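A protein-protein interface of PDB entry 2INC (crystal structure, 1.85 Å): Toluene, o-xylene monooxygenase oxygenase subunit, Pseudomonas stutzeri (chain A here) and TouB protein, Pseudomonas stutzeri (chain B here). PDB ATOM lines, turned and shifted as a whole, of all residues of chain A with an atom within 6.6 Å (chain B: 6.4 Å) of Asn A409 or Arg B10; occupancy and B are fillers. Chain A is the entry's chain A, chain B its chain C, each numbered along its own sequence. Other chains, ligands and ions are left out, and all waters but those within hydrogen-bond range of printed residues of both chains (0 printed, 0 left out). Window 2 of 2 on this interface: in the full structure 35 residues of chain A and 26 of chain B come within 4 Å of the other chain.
Printed residues of chain B within 4 Å of Gly A408: Arg B10 (2.9 Å).
Asn A409 touches one residue of chain B.
Printed residues of chain B within 4 Å of Trp A411: Phe B8, Glu B9, Arg B10 and Asp B11.
Printed residues of chain A within 4 Å of Phe B8: Trp A411 (3.4 Å).
Of chain A, only Gln A370, Pro A407, Gly A408, Asn A409 and Trp A411 come within 4 Å of Arg B10.
Printed residues of chain A within 4 Å of Asp B11: Pro A407, Trp A411 and Val A413.
Of the printed residues of chain A, Phe B12 touches Trp A368 (3.7 Å), Pro A407 (3.7 Å) and Val A413 (3.6 Å).
The nearest printed residue of chain B that does not touch Gln A370 is His B42 (4.1 Å).
The backbone carbonyl oxygen (O) of Arg B10 sits at hydrogen-bond distance from the backbone NH (N) of Gly A408 (2.9 Å).
The side-chain amide oxygen of Asn A409 is in hydrogen-bond range of the guanidinium group of Arg B10, at 2.6 Å.
The backbone carbonyl oxygen of Phe B8 sits at hydrogen-bond distance from the indole nitrogen of Trp A411, at 3.4 Å.
O of Asp B11 sits close to NE1 of Trp A411 (3.1 Å).
CZ3 of Trp A368 touches CB of Phe B12, 3.7 Å away.
Gln A370 touches Arg B10 (OE1 to NH2, 3.9 Å).
Cys A371 touches Arg B40 (CA to O, 3.7 Å).
Arg B10 touches Pro A407.
Asp B11 touches Pro A407.
CB of Pro A407 touches CB of Phe B12, 3.7 Å away.
Trp A411 touches Glu B9 (CE2 to CA, 3.7 Å).
N of Arg B10 touches CG of Trp A411, at 3.3 Å.
Asp B11 touches Val A413.
Val A413 touches Phe B12 (CG2 to O, 3.6 Å).
O of Asn A365 lies within hydrogen-bond range of NE2 of Gln A370 (3.3 Å).
The side-chain amide nitrogen (ND2) of Asn A409 is in hydrogen-bond range of the backbone carbonyl oxygen (O) of Asp A366, 2.7 Å away.
N of Glu B9 lies within hydrogen-bond range of O of Ile B79 (2.7 Å).
The side-chain carboxylate (OE1) of Glu B9 is in hydrogen-bond range of the backbone NH (N) of Phe B81.
The side-chain carboxylate of Asp B11 is in salt-bridge range of the guanidinium group of Arg B40 (3.0 Å).
Hydrophobic or aromatic side chains of chain B that line the printed part of chain A: Phe B12.
Among the printed residues, no Asp or Glu carboxylate lies within 4 Å of a Lys or Arg side-chain nitrogen of the other chain.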
ATOM      1  N   ASN A 365      10.278  28.017  -3.231  1.00  0.00           N
ATOM      2  CA  ASN A 365       9.459  26.828  -3.389  1.00  0.00           C
ATOM      3  C   ASN A 365       9.971  25.639  -2.667  1.00  0.00           C
ATOM      4  O   ASN A 365       9.179  24.800  -2.247  1.00  0.00           O
ATOM      5  CB  ASN A 365       9.181  26.521  -4.837  1.00  0.00           C
ATOM      6  CG  ASN A 365       7.934  27.219  -5.301  1.00  0.00           C
ATOM      7  OD1 ASN A 365       6.806  26.794  -4.993  1.00  0.00           O
ATOM      8  ND2 ASN A 365       8.117  28.351  -5.975  1.00  0.00           N
ATOM      9  N   ASP A 366      11.288  25.595  -2.472  1.00  0.00           N
ATOM     10  CA  ASP A 366      11.893  24.445  -1.817  1.00  0.00           C
ATOM     11  C   ASP A 366      12.118  24.619  -0.312  1.00  0.00           C
ATOM     12  O   ASP A 366      12.584  23.692   0.347  1.00  0.00           O
ATOM     13  CB  ASP A 366      13.156  24.020  -2.562  1.00  0.00           C
ATOM     14  CG  ASP A 366      12.827  23.420  -3.972  1.00  0.00           C
ATOM     15  OD1 ASP A 366      12.421  22.222  -4.083  1.00  0.00           O
ATOM     16  OD2 ASP A 366      12.959  24.173  -4.978  1.00  0.00           O
ATOM     17  N   THR A 367      11.754  25.800   0.217  1.00  0.00           N
ATOM     18  CA  THR A 367      11.685  26.054   1.672  1.00  0.00           C
ATOM     19  C   THR A 367      10.208  26.324   2.030  1.00  0.00           C
ATOM     20  O   THR A 367       9.459  25.388   2.294  1.00  0.00           O
ATOM     21  CB  THR A 367      12.564  27.237   2.107  1.00  0.00           C
ATOM     22  OG1 THR A 367      12.235  28.395   1.329  1.00  0.00           O
ATOM     23  CG2 THR A 367      14.061  26.913   1.915  1.00  0.00           C
ATOM     24  N   TRP A 368       9.788  27.593   2.003  1.00  0.00           N
ATOM     25  CA  TRP A 368       8.380  27.964   2.243  1.00  0.00           C
ATOM     26  C   TRP A 368       7.394  27.139   1.477  1.00  0.00           C
ATOM     27  O   TRP A 368       6.360  26.722   2.027  1.00  0.00           O
ATOM     28  CB  TRP A 368       8.171  29.477   1.994  1.00  0.00           C
ATOM     29  CG  TRP A 368       9.121  30.228   2.857  1.00  0.00           C
ATOM     30  CD1 TRP A 368      10.334  30.766   2.485  1.00  0.00           C
ATOM     31  CD2 TRP A 368       9.030  30.386   4.280  1.00  0.00           C
ATOM     32  NE1 TRP A 368      10.961  31.300   3.581  1.00  0.00           N
ATOM     33  CE2 TRP A 368      10.196  31.072   4.697  1.00  0.00           C
ATOM     34  CE3 TRP A 368       8.061  30.035   5.242  1.00  0.00           C
ATOM     35  CZ2 TRP A 368      10.425  31.415   6.028  1.00  0.00           C
ATOM     36  CZ3 TRP A 368       8.291  30.390   6.587  1.00  0.00           C
ATOM     37  CH2 TRP A 368       9.459  31.079   6.956  1.00  0.00           C
ATOM     38  N   GLN A 370       7.481  24.136   0.573  1.00  0.00           N
ATOM     39  CA  GLN A 370       7.251  22.823   1.192  1.00  0.00           C
ATOM     40  C   GLN A 370       6.040  22.802   2.132  1.00  0.00           C
ATOM     41  O   GLN A 370       5.238  21.894   2.059  1.00  0.00           O
ATOM     42  CB  GLN A 370       8.495  22.331   1.941  1.00  0.00           C
ATOM     43  CG  GLN A 370       9.717  22.155   1.075  1.00  0.00           C
ATOM     44  CD  GLN A 370       9.463  21.181  -0.020  1.00  0.00           C
ATOM     45  OE1 GLN A 370       9.415  19.973   0.225  1.00  0.00           O
ATOM     46  NE2 GLN A 370       9.219  21.687  -1.239  1.00  0.00           N
ATOM     47  N   CYS A 371       5.911  23.799   3.017  1.00  0.00           N
ATOM     48  CA  CYS A 371       4.837  23.765   3.997  1.00  0.00           C
ATOM     49  C   CYS A 371       3.554  24.004   3.266  1.00  0.00           C
ATOM     50  O   CYS A 371       2.516  23.374   3.540  1.00  0.00           O
ATOM     51  CB  CYS A 371       5.009  24.894   5.012  1.00  0.00           C
ATOM     52  SG  CYS A 371       6.504  24.821   5.986  1.00  0.00           S
ATOM     53  N   THR A 406      13.060  29.913   8.272  1.00  0.00           N
ATOM     54  CA  THR A 406      13.105  29.091   7.056  1.00  0.00           C
ATOM     55  C   THR A 406      12.818  27.595   7.321  1.00  0.00           C
ATOM     56  O   THR A 406      13.469  26.988   8.176  1.00  0.00           O
ATOM     57  CB  THR A 406      14.479  29.192   6.399  1.00  0.00           C
ATOM     58  OG1 THR A 406      14.895  30.563   6.366  1.00  0.00           O
ATOM     59  CG2 THR A 406      14.396  28.657   4.986  1.00  0.00           C
ATOM     60  N   PRO A 407      11.824  27.018   6.611  1.00  0.00           N
ATOM     61  CA  PRO A 407      11.452  25.620   6.736  1.00  0.00           C
ATOM     62  C   PRO A 407      11.997  24.785   5.559  1.00  0.00           C
ATOM     63  O   PRO A 407      12.823  25.265   4.782  1.00  0.00           O
ATOM     64  CB  PRO A 407       9.940  25.685   6.601  1.00  0.00           C
ATOM     65  CG  PRO A 407       9.712  26.825   5.547  1.00  0.00           C
ATOM     66  CD  PRO A 407      10.979  27.701   5.613  1.00  0.00           C
ATOM     67  N   GLY A 408      11.507  23.558   5.421  1.00  0.00           N
ATOM     68  CA  GLY A 408      11.724  22.759   4.206  1.00  0.00           C
ATOM     69  C   GLY A 408      13.174  22.381   4.017  1.00  0.00           C
ATOM     70  O   GLY A 408      13.864  22.032   4.976  1.00  0.00           O
ATOM     71  N   ASN A 409      13.654  22.512   2.788  1.00  0.00           N
ATOM     72  CA  ASN A 409      14.977  21.998   2.436  1.00  0.00           C
ATOM     73  C   ASN A 409      16.168  22.794   2.953  1.00  0.00           C
ATOM     74  O   ASN A 409      17.307  22.391   2.743  1.00  0.00           O
ATOM     75  CB  ASN A 409      15.069  21.739   0.921  1.00  0.00           C
ATOM     76  CG  ASN A 409      13.988  20.758   0.432  1.00  0.00           C
ATOM     77  OD1 ASN A 409      13.924  19.606   0.883  1.00  0.00           O
ATOM     78  ND2 ASN A 409      13.121  21.220  -0.477  1.00  0.00           N
ATOM     79  N   LYS A 410      15.924  23.939   3.597  1.00  0.00           N
ATOM     80  CA  LYS A 410      16.998  24.692   4.275  1.00  0.00           C
ATOM     81  C   LYS A 410      16.534  25.120   5.667  1.00  0.00           C
ATOM     82  O   LYS A 410      16.667  26.296   6.056  1.00  0.00           O
ATOM     83  CB  LYS A 410      17.440  25.910   3.453  1.00  0.00           C
ATOM     84  CG  LYS A 410      17.965  25.564   2.038  1.00  0.00           C
ATOM     85  CD  LYS A 410      19.150  26.444   1.632  1.00  0.00           C
ATOM     86  CE  LYS A 410      18.694  27.808   1.053  1.00  0.00           C
ATOM     87  NZ  LYS A 410      19.830  28.603   0.451  1.00  0.00           N
ATOM     88  N   TRP A 411      15.973  24.162   6.404  1.00  0.00           N
ATOM     89  CA  TRP A 411      15.449  24.379   7.744  1.00  0.00           C
ATOM     90  C   TRP A 411      16.424  25.135   8.627  1.00  0.00           C
ATOM     91  O   TRP A 411      17.574  24.728   8.789  1.00  0.00           O
ATOM     92  CB  TRP A 411      15.109  23.039   8.374  1.00  0.00           C
ATOM     93  CG  TRP A 411      14.452  23.160   9.687  1.00  0.00           C
ATOM     94  CD1 TRP A 411      13.320  23.885   9.982  1.00  0.00           C
ATOM     95  CD2 TRP A 411      14.866  22.539  10.918  1.00  0.00           C
ATOM     96  NE1 TRP A 411      13.012  23.749  11.319  1.00  0.00           N
ATOM     97  CE2 TRP A 411      13.939  22.933  11.918  1.00  0.00           C
ATOM     98  CE3 TRP A 411      15.910  21.664  11.264  1.00  0.00           C
ATOM     99  CZ2 TRP A 411      14.018  22.475  13.249  1.00  0.00           C
ATOM    100  CZ3 TRP A 411      16.003  21.214  12.607  1.00  0.00           C
ATOM    101  CH2 TRP A 411      15.059  21.627  13.581  1.00  0.00           C
ATOM    102  N   VAL A 413      15.128  27.221  11.731  1.00  0.00           N
ATOM    103  CA  VAL A 413      14.327  27.845  12.787  1.00  0.00           C
ATOM    104  C   VAL A 413      15.122  27.724  14.068  1.00  0.00           C
ATOM    105  O   VAL A 413      15.584  26.638  14.399  1.00  0.00           O
ATOM    106  CB  VAL A 413      12.953  27.154  12.951  1.00  0.00           C
ATOM    107  CG1 VAL A 413      12.092  27.824  14.055  1.00  0.00           C
ATOM    108  CG2 VAL A 413      12.232  27.117  11.635  1.00  0.00           C
ATOM    109  N   PHE B   8      10.243  21.446  15.134  1.00  0.00           N
ATOM    110  CA  PHE B   8      10.174  20.221  14.359  1.00  0.00           C
ATOM    111  C   PHE B   8      10.944  20.366  13.047  1.00  0.00           C
ATOM    112  O   PHE B   8      10.836  21.417  12.372  1.00  0.00           O
ATOM    113  CB  PHE B   8       8.717  19.850  14.111  1.00  0.00           C
ATOM    114  CG  PHE B   8       8.530  18.385  13.819  1.00  0.00           C
ATOM    115  CD1 PHE B   8       8.161  17.505  14.841  1.00  0.00           C
ATOM    116  CD2 PHE B   8       8.745  17.878  12.541  1.00  0.00           C
ATOM    117  CE1 PHE B   8       7.983  16.131  14.587  1.00  0.00           C
ATOM    118  CE2 PHE B   8       8.587  16.501  12.289  1.00  0.00           C
ATOM    119  CZ  PHE B   8       8.222  15.642  13.319  1.00  0.00           C
ATOM    120  N   GLU B   9      11.739  19.344  12.677  1.00  0.00           N
ATOM    121  CA  GLU B   9      12.617  19.502  11.519  1.00  0.00           C
ATOM    122  C   GLU B   9      11.779  19.765  10.292  1.00  0.00           C
ATOM    123  O   GLU B   9      10.715  19.139  10.107  1.00  0.00           O
ATOM    124  CB  GLU B   9      13.506  18.281  11.291  1.00  0.00           C
ATOM    125  CG  GLU B   9      14.390  18.404  10.066  1.00  0.00           C
ATOM    126  CD  GLU B   9      15.433  17.275   9.981  1.00  0.00           C
ATOM    127  OE1 GLU B   9      15.414  16.345  10.823  1.00  0.00           O
ATOM    128  OE2 GLU B   9      16.264  17.327   9.056  1.00  0.00           O
ATOM    129  N   ARG B  10      12.232  20.748   9.510  1.00  0.00           N
ATOM    130  CA  ARG B  10      11.563  21.172   8.258  1.00  0.00           C
ATOM    131  C   ARG B  10      10.255  21.964   8.408  1.00  0.00           C
ATOM    132  O   ARG B  10       9.713  22.436   7.399  1.00  0.00           O
ATOM    133  CB  ARG B  10      11.326  19.962   7.346  1.00  0.00           C
ATOM    134  CG  ARG B  10      12.611  19.233   7.005  1.00  0.00           C
ATOM    135  CD  ARG B  10      12.272  18.011   6.202  1.00  0.00           C
ATOM    136  NE  ARG B  10      11.857  18.451   4.882  1.00  0.00           N
ATOM    137  CZ  ARG B  10      12.700  18.679   3.881  1.00  0.00           C
ATOM    138  NH1 ARG B  10      14.015  18.451   4.043  1.00  0.00           N
ATOM    139  NH2 ARG B  10      12.222  19.121   2.721  1.00  0.00           N
ATOM    140  N   ASP B  11       9.712  22.047   9.626  1.00  0.00           N
ATOM    141  CA  ASP B  11       8.637  23.007   9.923  1.00  0.00           C
ATOM    142  C   ASP B  11       9.207  24.461   9.943  1.00  0.00           C
ATOM    143  O   ASP B  11      10.438  24.669   9.886  1.00  0.00           O
ATOM    144  CB  ASP B  11       7.958  22.673  11.249  1.00  0.00           C
ATOM    145  CG  ASP B  11       6.470  23.071  11.269  1.00  0.00           C
ATOM    146  OD1 ASP B  11       6.035  23.945  10.476  1.00  0.00           O
ATOM    147  OD2 ASP B  11       5.714  22.517  12.096  1.00  0.00           O
ATOM    148  N   PHE B  12       8.323  25.453  10.076  1.00  0.00           N
ATOM    149  CA  PHE B  12       8.736  26.877  10.021  1.00  0.00           C
ATOM    150  C   PHE B  12       8.560  27.569  11.350  1.00  0.00           C
ATOM    151  O   PHE B  12       8.968  28.719  11.478  1.00  0.00           O
ATOM    152  CB  PHE B  12       7.910  27.650   8.988  1.00  0.00           C
ATOM    153  CG  PHE B  12       6.577  28.115   9.517  1.00  0.00           C
ATOM    154  CD1 PHE B  12       6.355  29.482   9.815  1.00  0.00           C
ATOM    155  CD2 PHE B  12       5.554  27.208   9.766  1.00  0.00           C
ATOM    156  CE1 PHE B  12       5.129  29.933  10.311  1.00  0.00           C
ATOM    157  CE2 PHE B  12       4.299  27.667  10.243  1.00  0.00           C
ATOM    158  CZ  PHE B  12       4.106  29.043  10.529  1.00  0.00           C
ATOM    159  N   ARG B  40       2.043  20.790   7.796  1.00  0.00           N
ATOM    160  CA  ARG B  40       3.164  21.221   7.231  1.00  0.00           C
ATOM    161  C   ARG B  40       4.470  20.477   6.984  1.00  0.00           C
ATOM    162  O   ARG B  40       5.265  21.084   6.450  1.00  0.00           O
ATOM    163  CB  ARG B  40       3.523  22.427   7.945  1.00  0.00           C
ATOM    164  CG  ARG B  40       2.552  23.333   8.046  1.00  0.00           C
ATOM    165  CD  ARG B  40       2.889  24.477   9.028  1.00  0.00           C
ATOM    166  NE  ARG B  40       1.881  24.465  10.006  1.00  0.00           N
ATOM    167  CZ  ARG B  40       1.970  24.175  11.245  1.00  0.00           C
ATOM    168  NH1 ARG B  40       3.071  23.997  11.887  1.00  0.00           N
ATOM    169  NH2 ARG B  40       0.923  24.267  11.784  1.00  0.00           N
ATOM    170  N   VAL B  41       4.731  19.240   7.336  1.00  0.00           N
ATOM    171  CA  VAL B  41       5.946  18.531   6.979  1.00  0.00           C
ATOM    172  C   VAL B  41       5.462  17.170   6.450  1.00  0.00           C
ATOM    173  O   VAL B  41       4.481  16.604   6.987  1.00  0.00           O
ATOM    174  CB  VAL B  41       6.845  18.345   8.219  1.00  0.00           C
ATOM    175  CG1 VAL B  41       8.142  17.672   7.821  1.00  0.00           C
ATOM    176  CG2 VAL B  41       7.129  19.693   8.892  1.00  0.00           C
ATOM    177  N   HIS B  42       6.096  16.678   5.377  1.00  0.00           N
ATOM    178  CA  HIS B  42       5.759  15.347   4.820  1.00  0.00           C
ATOM    179  C   HIS B  42       6.396  14.303   5.716  1.00  0.00           C
ATOM    180  O   HIS B  42       7.495  14.527   6.199  1.00  0.00           O
ATOM    181  CB  HIS B  42       6.337  15.135   3.421  1.00  0.00           C
ATOM    182  CG  HIS B  42       5.865  16.111   2.385  1.00  0.00           C
ATOM    183  ND1 HIS B  42       6.575  17.252   2.056  1.00  0.00           N
ATOM    184  CD2 HIS B  42       4.765  16.107   1.588  1.00  0.00           C
ATOM    185  CE1 HIS B  42       5.934  17.905   1.100  1.00  0.00           C
ATOM    186  NE2 HIS B  42       4.829  17.236   0.803  1.00  0.00           N
ATOM    187  N   GLN B  44       8.510  10.909   6.789  1.00  0.00           N
ATOM    188  CA  GLN B  44       9.721  10.278   6.291  1.00  0.00           C
ATOM    189  C   GLN B  44       9.820   8.900   6.948  1.00  0.00           C
ATOM    190  O   GLN B  44      10.551   8.748   7.938  1.00  0.00           O
ATOM    191  CB  GLN B  44      10.955  11.100   6.630  1.00  0.00           C
ATOM    192  CG  GLN B  44      11.056  12.416   5.906  1.00  0.00           C
ATOM    193  CD  GLN B  44      12.428  13.058   6.054  1.00  0.00           C
ATOM    194  OE1 GLN B  44      13.451  12.368   6.132  1.00  0.00           O
ATOM    195  NE2 GLN B  44      12.457  14.396   6.098  1.00  0.00           N
ATOM    196  N   ILE B  79      13.132  18.326  17.025  1.00  0.00           N
ATOM    197  CA  ILE B  79      12.653  16.982  16.731  1.00  0.00           C
ATOM    198  C   ILE B  79      13.134  16.751  15.323  1.00  0.00           C
ATOM    199  O   ILE B  79      12.682  17.416  14.355  1.00  0.00           O
ATOM    200  CB  ILE B  79      11.119  16.804  16.871  1.00  0.00           C
ATOM    201  CG1 ILE B  79      10.628  17.284  18.229  1.00  0.00           C
ATOM    202  CG2 ILE B  79      10.737  15.311  16.812  1.00  0.00           C
ATOM    203  CD1 ILE B  79      10.475  18.760  18.272  1.00  0.00           C
ATOM    204  N   PHE B  81      14.720  14.110  12.063  1.00  0.00           N
ATOM    205  CA  PHE B  81      14.710  12.826  11.335  1.00  0.00           C
ATOM    206  C   PHE B  81      16.097  12.203  11.349  1.00  0.00           C
ATOM    207  O   PHE B  81      17.075  12.790  10.837  1.00  0.00           O
ATOM    208  CB  PHE B  81      14.269  13.022   9.884  1.00  0.00           C
ATOM    209  CG  PHE B  81      12.891  13.555   9.751  1.00  0.00           C
ATOM    210  CD1 PHE B  81      11.805  12.710   9.794  1.00  0.00           C
ATOM    211  CD2 PHE B  81      12.678  14.921   9.626  1.00  0.00           C
ATOM    212  CE1 PHE B  81      10.515  13.193   9.697  1.00  0.00           C
ATOM    213  CE2 PHE B  81      11.404  15.415   9.515  1.00  0.00           C
ATOM    214  CZ  PHE B  81      10.308  14.554   9.558  1.00  0.00           C
